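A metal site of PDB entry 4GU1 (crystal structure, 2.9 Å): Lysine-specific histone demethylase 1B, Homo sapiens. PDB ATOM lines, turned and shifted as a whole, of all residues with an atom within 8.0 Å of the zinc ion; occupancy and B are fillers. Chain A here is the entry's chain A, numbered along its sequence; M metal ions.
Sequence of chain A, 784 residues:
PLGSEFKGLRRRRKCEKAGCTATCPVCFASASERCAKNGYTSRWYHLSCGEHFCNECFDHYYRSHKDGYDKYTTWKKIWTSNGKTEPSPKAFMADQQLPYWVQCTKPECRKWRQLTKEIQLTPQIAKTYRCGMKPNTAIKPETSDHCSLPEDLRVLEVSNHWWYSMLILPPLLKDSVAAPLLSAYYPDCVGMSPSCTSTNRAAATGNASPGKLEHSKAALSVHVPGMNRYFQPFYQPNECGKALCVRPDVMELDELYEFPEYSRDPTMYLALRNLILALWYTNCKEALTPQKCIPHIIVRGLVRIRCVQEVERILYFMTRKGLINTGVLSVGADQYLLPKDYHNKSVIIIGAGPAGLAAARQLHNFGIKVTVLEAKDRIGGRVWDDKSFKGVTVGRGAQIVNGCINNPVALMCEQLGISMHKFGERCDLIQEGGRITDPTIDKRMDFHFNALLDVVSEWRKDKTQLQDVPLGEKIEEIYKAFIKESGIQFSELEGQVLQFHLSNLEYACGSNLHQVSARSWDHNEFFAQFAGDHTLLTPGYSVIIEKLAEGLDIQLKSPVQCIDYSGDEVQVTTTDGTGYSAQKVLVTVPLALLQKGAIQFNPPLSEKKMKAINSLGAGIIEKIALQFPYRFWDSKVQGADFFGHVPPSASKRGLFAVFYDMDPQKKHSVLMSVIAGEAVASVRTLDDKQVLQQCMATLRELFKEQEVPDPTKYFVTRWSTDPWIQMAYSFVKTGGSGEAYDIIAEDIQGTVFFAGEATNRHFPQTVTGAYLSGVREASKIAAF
SG of Cys 35 sits close to O of Ala 29, 3.5 Å away.
The backbone NH of Ala 29 sits close to the side-chain sulfur of Cys 27 (3.7 Å).
The backbone NH (N) of Cys 27 sits at hydrogen-bond distance from the backbone carbonyl oxygen (O) of Lys 37.
The side-chain sulfur of Cys 35 lies close to the backbone NH of Lys 37, 3.8 Å away.
SG of Cys 57 lies close to O of Ala 29.
The side-chain sulfur (SG) of Cys 54 sits close to the backbone NH (N) of Glu 56, at 3.5 Å.
The zinc ion is bound by the side-chain sulfur of Cys 54 (2.3 Å), the side-chain sulfur of Cys 57 (2.3 Å), the side-chain sulfur of Cys 35 (2.5 Å) and the side-chain sulfur of Cys 27 (2.6 Å).
The zinc ion has four donor atoms within binding distance.
Residues that only touch the zinc ion: Ala 29 (3.5 Å).
Five residues have an atom within 4 Å of the zinc ion: Cys 27, Ala 29, Cys 35, Cys 54 and Cys 57.
The nearest printed residue that does not touch the zinc ion is Ala 36 (4.03 Å).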
ATOM      1  N   VAL A  26      32.500 -36.820 -10.525  1.00  0.00           N
ATOM      2  CA  VAL A  26      32.217 -35.555 -11.171  1.00  0.00           C
ATOM      3  C   VAL A  26      30.780 -35.169 -10.794  1.00  0.00           C
ATOM      4  O   VAL A  26      30.091 -35.939 -10.108  1.00  0.00           O
ATOM      5  CB  VAL A  26      32.493 -35.639 -12.708  1.00  0.00           C
ATOM      6  CG1 VAL A  26      33.369 -36.853 -13.029  1.00  0.00           C
ATOM      7  CG2 VAL A  26      31.220 -35.632 -13.557  1.00  0.00           C
ATOM      8  N   CYS A  27      30.328 -33.977 -11.181  1.00  0.00           N
ATOM      9  CA  CYS A  27      28.942 -33.598 -10.973  1.00  0.00           C
ATOM     10  C   CYS A  27      28.193 -33.580 -12.313  1.00  0.00           C
ATOM     11  O   CYS A  27      28.769 -33.249 -13.338  1.00  0.00           O
ATOM     12  CB  CYS A  27      28.862 -32.237 -10.291  1.00  0.00           C
ATOM     13  SG  CYS A  27      27.221 -31.720  -9.811  1.00  0.00           S
ATOM     14  N   PHE A  28      26.916 -33.956 -12.297  1.00  0.00           N
ATOM     15  CA  PHE A  28      26.168 -34.130 -13.545  1.00  0.00           C
ATOM     16  C   PHE A  28      25.309 -32.905 -13.863  1.00  0.00           C
ATOM     17  O   PHE A  28      24.869 -32.712 -15.005  1.00  0.00           O
ATOM     18  CB  PHE A  28      25.271 -35.371 -13.473  1.00  0.00           C
ATOM     19  CG  PHE A  28      23.966 -35.134 -12.776  1.00  0.00           C
ATOM     20  CD1 PHE A  28      23.883 -35.193 -11.386  1.00  0.00           C
ATOM     21  CD2 PHE A  28      22.815 -34.838 -13.503  1.00  0.00           C
ATOM     22  CE1 PHE A  28      22.663 -34.963 -10.742  1.00  0.00           C
ATOM     23  CE2 PHE A  28      21.607 -34.604 -12.846  1.00  0.00           C
ATOM     24  CZ  PHE A  28      21.528 -34.675 -11.472  1.00  0.00           C
ATOM     25  N   ALA A  29      25.040 -32.116 -12.834  1.00  0.00           N
ATOM     26  CA  ALA A  29      24.157 -30.952 -12.945  1.00  0.00           C
ATOM     27  C   ALA A  29      24.908 -29.646 -12.686  1.00  0.00           C
ATOM     28  O   ALA A  29      25.003 -29.199 -11.541  1.00  0.00           O
ATOM     29  CB  ALA A  29      23.006 -31.089 -11.967  1.00  0.00           C
ATOM     30  N   SER A  30      25.437 -29.031 -13.740  1.00  0.00           N
ATOM     31  CA  SER A  30      25.937 -27.667 -13.581  1.00  0.00           C
ATOM     32  C   SER A  30      24.719 -26.776 -13.391  1.00  0.00           C
ATOM     33  O   SER A  30      24.218 -26.164 -14.325  1.00  0.00           O
ATOM     34  CB  SER A  30      26.764 -27.232 -14.797  1.00  0.00           C
ATOM     35  OG  SER A  30      26.080 -27.486 -16.016  1.00  0.00           O
ATOM     36  N   ALA A  31      24.219 -26.740 -12.146  1.00  0.00           N
ATOM     37  CA  ALA A  31      22.925 -26.138 -11.862  1.00  0.00           C
ATOM     38  C   ALA A  31      23.051 -24.886 -11.006  1.00  0.00           C
ATOM     39  O   ALA A  31      22.210 -23.993 -11.085  1.00  0.00           O
ATOM     40  CB  ALA A  31      21.994 -27.154 -11.191  1.00  0.00           C
ATOM     41  N   SER A  32      24.095 -24.839 -10.189  1.00  0.00           N
ATOM     42  CA  SER A  32      24.425 -23.642  -9.427  1.00  0.00           C
ATOM     43  C   SER A  32      25.551 -22.919 -10.169  1.00  0.00           C
ATOM     44  O   SER A  32      26.125 -23.462 -11.120  1.00  0.00           O
ATOM     45  CB  SER A  32      24.865 -23.997  -7.994  1.00  0.00           C
ATOM     46  OG  SER A  32      24.808 -22.875  -7.135  1.00  0.00           O
ATOM     47  N   GLU A  33      25.847 -21.691  -9.751  1.00  0.00           N
ATOM     48  CA  GLU A  33      26.961 -20.949 -10.337  1.00  0.00           C
ATOM     49  C   GLU A  33      28.270 -21.592  -9.920  1.00  0.00           C
ATOM     50  O   GLU A  33      29.214 -21.697 -10.702  1.00  0.00           O
ATOM     51  CB  GLU A  33      26.926 -19.481  -9.889  1.00  0.00           C
ATOM     52  CG  GLU A  33      25.992 -18.605 -10.706  1.00  0.00           C
ATOM     53  CD  GLU A  33      26.407 -18.516 -12.173  1.00  0.00           C
ATOM     54  OE1 GLU A  33      27.614 -18.628 -12.461  1.00  0.00           O
ATOM     55  OE2 GLU A  33      25.511 -18.346 -13.034  1.00  0.00           O
ATOM     56  N   ARG A  34      28.301 -22.045  -8.671  1.00  0.00           N
ATOM     57  CA  ARG A  34      29.479 -22.621  -8.056  1.00  0.00           C
ATOM     58  C   ARG A  34      29.414 -24.148  -8.009  1.00  0.00           C
ATOM     59  O   ARG A  34      29.718 -24.766  -6.975  1.00  0.00           O
ATOM     60  CB  ARG A  34      29.658 -22.048  -6.650  1.00  0.00           C
ATOM     61  CG  ARG A  34      29.417 -20.548  -6.580  1.00  0.00           C
ATOM     62  CD  ARG A  34      28.662 -20.175  -5.306  1.00  0.00           C
ATOM     63  NE  ARG A  34      27.341 -20.800  -5.241  1.00  0.00           N
ATOM     64  CZ  ARG A  34      26.683 -21.049  -4.105  1.00  0.00           C
ATOM     65  NH1 ARG A  34      27.227 -20.745  -2.935  1.00  0.00           N
ATOM     66  NH2 ARG A  34      25.481 -21.623  -4.149  1.00  0.00           N
ATOM     67  N   CYS A  35      29.001 -24.760  -9.118  1.00  0.00           N
ATOM     68  CA  CYS A  35      29.076 -26.214  -9.275  1.00  0.00           C
ATOM     69  C   CYS A  35      30.552 -26.571  -9.127  1.00  0.00           C
ATOM     70  O   CYS A  35      31.426 -25.903  -9.686  1.00  0.00           O
ATOM     71  CB  CYS A  35      28.531 -26.659 -10.643  1.00  0.00           C
ATOM     72  SG  CYS A  35      28.372 -28.484 -10.963  1.00  0.00           S
ATOM     73  N   ALA A  36      30.816 -27.619  -8.348  1.00  0.00           N
ATOM     74  CA  ALA A  36      32.169 -28.063  -8.081  1.00  0.00           C
ATOM     75  C   ALA A  36      32.752 -28.929  -9.204  1.00  0.00           C
ATOM     76  O   ALA A  36      33.768 -29.573  -9.002  1.00  0.00           O
ATOM     77  CB  ALA A  36      32.234 -28.784  -6.756  1.00  0.00           C
ATOM     78  N   LYS A  37      32.095 -28.921 -10.374  1.00  0.00           N
ATOM     79  CA  LYS A  37      32.480 -29.694 -11.573  1.00  0.00           C
ATOM     80  C   LYS A  37      33.196 -31.024 -11.286  1.00  0.00           C
ATOM     81  O   LYS A  37      32.540 -32.028 -10.960  1.00  0.00           O
ATOM     82  CB  LYS A  37      33.314 -28.857 -12.545  1.00  0.00           C
ATOM     83  CG  LYS A  37      32.962 -27.375 -12.632  1.00  0.00           C
ATOM     84  CD  LYS A  37      31.608 -27.093 -13.266  1.00  0.00           C
ATOM     85  CE  LYS A  37      31.458 -25.594 -13.459  1.00  0.00           C
ATOM     86  NZ  LYS A  37      30.039 -25.137 -13.395  1.00  0.00           N
ATOM     87  N   ASN A  38      34.523 -31.044 -11.418  1.00  0.00           N
ATOM     88  CA  ASN A  38      35.321 -32.198 -10.965  1.00  0.00           C
ATOM     89  C   ASN A  38      36.158 -31.887  -9.730  1.00  0.00           C
ATOM     90  O   ASN A  38      36.835 -32.765  -9.193  1.00  0.00           O
ATOM     91  CB  ASN A  38      36.217 -32.756 -12.063  1.00  0.00           C
ATOM     92  CG  ASN A  38      36.465 -31.768 -13.165  1.00  0.00           C
ATOM     93  OD1 ASN A  38      35.802 -31.783 -14.198  1.00  0.00           O
ATOM     94  ND2 ASN A  38      37.426 -30.873 -12.944  1.00  0.00           N
ATOM     95  N   THR A  41      34.073 -30.564  -3.072  1.00  0.00           N
ATOM     96  CA  THR A  41      32.862 -30.150  -2.377  1.00  0.00           C
ATOM     97  C   THR A  41      32.822 -30.717  -0.956  1.00  0.00           C
ATOM     98  O   THR A  41      33.458 -31.731  -0.653  1.00  0.00           O
ATOM     99  CB  THR A  41      31.572 -30.518  -3.161  1.00  0.00           C
ATOM    100  OG1 THR A  41      30.412 -30.025  -2.473  1.00  0.00           O
ATOM    101  CG2 THR A  41      31.456 -32.020  -3.348  1.00  0.00           C
ATOM    102  N   TRP A  44      29.608 -35.027  -1.362  1.00  0.00           N
ATOM    103  CA  TRP A  44      29.070 -35.592  -2.588  1.00  0.00           C
ATOM    104  C   TRP A  44      27.764 -36.315  -2.320  1.00  0.00           C
ATOM    105  O   TRP A  44      27.546 -36.847  -1.225  1.00  0.00           O
ATOM    106  CB  TRP A  44      30.083 -36.543  -3.241  1.00  0.00           C
ATOM    107  CG  TRP A  44      31.133 -35.831  -4.014  1.00  0.00           C
ATOM    108  CD1 TRP A  44      32.461 -35.765  -3.715  1.00  0.00           C
ATOM    109  CD2 TRP A  44      30.957 -35.082  -5.222  1.00  0.00           C
ATOM    110  NE1 TRP A  44      33.121 -35.025  -4.668  1.00  0.00           N
ATOM    111  CE2 TRP A  44      32.216 -34.594  -5.597  1.00  0.00           C
ATOM    112  CE3 TRP A  44      29.849 -34.775  -6.020  1.00  0.00           C
ATOM    113  CZ2 TRP A  44      32.399 -33.809  -6.733  1.00  0.00           C
ATOM    114  CZ3 TRP A  44      30.042 -34.010  -7.154  1.00  0.00           C
ATOM    115  CH2 TRP A  44      31.310 -33.533  -7.496  1.00  0.00           C
ATOM    116  N   HIS A  52      26.715 -38.626  -9.596  1.00  0.00           N
ATOM    117  CA  HIS A  52      26.776 -37.868  -8.349  1.00  0.00           C
ATOM    118  C   HIS A  52      26.423 -36.397  -8.574  1.00  0.00           C
ATOM    119  O   HIS A  52      26.465 -35.903  -9.715  1.00  0.00           O
ATOM    120  CB  HIS A  52      28.165 -37.943  -7.724  1.00  0.00           C
ATOM    121  CG  HIS A  52      28.650 -39.337  -7.476  1.00  0.00           C
ATOM    122  ND1 HIS A  52      29.134 -40.152  -8.481  1.00  0.00           N
ATOM    123  CD2 HIS A  52      28.761 -40.056  -6.326  1.00  0.00           C
ATOM    124  CE1 HIS A  52      29.491 -41.320  -7.959  1.00  0.00           C
ATOM    125  NE2 HIS A  52      29.277 -41.287  -6.657  1.00  0.00           N
ATOM    126  N   PHE A  53      26.080 -35.698  -7.500  1.00  0.00           N
ATOM    127  CA  PHE A  53      25.923 -34.248  -7.575  1.00  0.00           C
ATOM    128  C   PHE A  53      26.449 -33.553  -6.317  1.00  0.00           C
ATOM    129  O   PHE A  53      26.363 -34.106  -5.219  1.00  0.00           O
ATOM    130  CB  PHE A  53      24.491 -33.846  -7.928  1.00  0.00           C
ATOM    131  CG  PHE A  53      23.476 -34.108  -6.852  1.00  0.00           C
ATOM    132  CD1 PHE A  53      23.184 -33.147  -5.907  1.00  0.00           C
ATOM    133  CD2 PHE A  53      22.800 -35.307  -6.814  1.00  0.00           C
ATOM    134  CE1 PHE A  53      22.245 -33.380  -4.921  1.00  0.00           C
ATOM    135  CE2 PHE A  53      21.852 -35.544  -5.827  1.00  0.00           C
ATOM    136  CZ  PHE A  53      21.568 -34.579  -4.883  1.00  0.00           C
ATOM    137  N   CYS A  54      26.980 -32.342  -6.501  1.00  0.00           N
ATOM    138  CA  CYS A  54      27.729 -31.637  -5.463  1.00  0.00           C
ATOM    139  C   CYS A  54      26.837 -30.942  -4.443  1.00  0.00           C
ATOM    140  O   CYS A  54      25.634 -30.823  -4.647  1.00  0.00           O
ATOM    141  CB  CYS A  54      28.630 -30.595  -6.096  1.00  0.00           C
ATOM    142  SG  CYS A  54      27.715 -29.148  -6.658  1.00  0.00           S
ATOM    143  N   ASN A  55      27.433 -30.465  -3.355  1.00  0.00           N
ATOM    144  CA  ASN A  55      26.656 -29.839  -2.292  1.00  0.00           C
ATOM    145  C   ASN A  55      25.980 -28.525  -2.681  1.00  0.00           C
ATOM    146  O   ASN A  55      24.975 -28.154  -2.101  1.00  0.00           O
ATOM    147  CB  ASN A  55      27.514 -29.659  -1.026  1.00  0.00           C
ATOM    148  CG  ASN A  55      26.670 -29.527   0.234  1.00  0.00           C
ATOM    149  OD1 ASN A  55      26.718 -30.394   1.117  1.00  0.00           O
ATOM    150  ND2 ASN A  55      25.915 -28.437   0.344  1.00  0.00           N
ATOM    151  N   GLU A  56      26.542 -27.823  -3.665  1.00  0.00           N
ATOM    152  CA  GLU A  56      25.968 -26.535  -4.054  1.00  0.00           C
ATOM    153  C   GLU A  56      24.715 -26.715  -4.909  1.00  0.00           C
ATOM    154  O   GLU A  56      23.819 -25.867  -4.882  1.00  0.00           O
ATOM    155  CB  GLU A  56      26.996 -25.646  -4.780  1.00  0.00           C
ATOM    156  CG  GLU A  56      28.066 -25.039  -3.869  1.00  0.00           C
ATOM    157  CD  GLU A  56      29.256 -25.974  -3.633  1.00  0.00           C
ATOM    158  OE1 GLU A  56      30.275 -25.841  -4.341  1.00  0.00           O
ATOM    159  OE2 GLU A  56      29.162 -26.843  -2.739  1.00  0.00           O
ATOM    160  N   CYS A  57      24.649 -27.806  -5.654  1.00  0.00           N
ATOM    161  CA  CYS A  57      23.472 -28.111  -6.458  1.00  0.00           C
ATOM    162  C   CYS A  57      22.360 -28.741  -5.606  1.00  0.00           C
ATOM    163  O   CYS A  57      21.179 -28.656  -5.941  1.00  0.00           O
ATOM    164  CB  CYS A  57      23.852 -29.009  -7.636  1.00  0.00           C
ATOM    165  SG  CYS A  57      25.150 -28.280  -8.689  1.00  0.00           S
ATOM    166  N   PHE A  58      22.757 -29.348  -4.500  1.00  0.00           N
ATOM    167  CA  PHE A  58      21.832 -29.788  -3.470  1.00  0.00           C
ATOM    168  C   PHE A  58      21.129 -28.548  -2.901  1.00  0.00           C
ATOM    169  O   PHE A  58      19.895 -28.467  -2.866  1.00  0.00           O
ATOM    170  CB  PHE A  58      22.608 -30.517  -2.367  1.00  0.00           C
ATOM    171  CG  PHE A  58      21.752 -30.976  -1.214  1.00  0.00           C
ATOM    172  CD1 PHE A  58      21.082 -32.191  -1.273  1.00  0.00           C
ATOM    173  CD2 PHE A  58      21.655 -30.214  -0.061  1.00  0.00           C
ATOM    174  CE1 PHE A  58      20.310 -32.617  -0.211  1.00  0.00           C
ATOM    175  CE2 PHE A  58      20.874 -30.644   1.003  1.00  0.00           C
ATOM    176  CZ  PHE A  58      20.198 -31.851   0.924  1.00  0.00           C
ATOM    177  N   HIS A  60      21.120 -25.533  -4.119  1.00  0.00           N
ATOM    178  CA  HIS A  60      20.503 -24.756  -5.186  1.00  0.00           C
ATOM    179  C   HIS A  60      19.022 -25.052  -5.349  1.00  0.00           C
ATOM    180  O   HIS A  60      18.267 -24.210  -5.840  1.00  0.00           O
ATOM    181  CB  HIS A  60      21.255 -24.993  -6.515  1.00  0.00           C
ATOM    182  CG  HIS A  60      20.612 -24.360  -7.711  1.00  0.00           C
ATOM    183  ND1 HIS A  60      19.432 -24.829  -8.260  1.00  0.00           N
ATOM    184  CD2 HIS A  60      20.993 -23.310  -8.475  1.00  0.00           C
ATOM    185  CE1 HIS A  60      19.124 -24.090  -9.315  1.00  0.00           C
ATOM    186  NE2 HIS A  60      20.051 -23.167  -9.461  1.00  0.00           N
ATOM    187  N   MET A  93      16.274 -35.283  -8.378  1.00  0.00           N
ATOM    188  CA  MET A  93      17.332 -35.303  -9.366  1.00  0.00           C
ATOM    189  C   MET A  93      17.105 -36.482 -10.303  1.00  0.00           C
ATOM    190  O   MET A  93      17.244 -36.378 -11.517  1.00  0.00           O
ATOM    191  CB  MET A  93      18.723 -35.380  -8.727  1.00  0.00           C
ATOM    192  CG  MET A  93      19.129 -34.192  -7.835  1.00  0.00           C
ATOM    193  SD  MET A  93      19.137 -32.583  -8.680  1.00  0.00           S
ATOM    194  CE  MET A  93      20.846 -32.397  -9.180  1.00  0.00           C
HETATM  195 ZN    ZN M   1      27.195 -29.317  -8.865  1.00  0.00          ZN
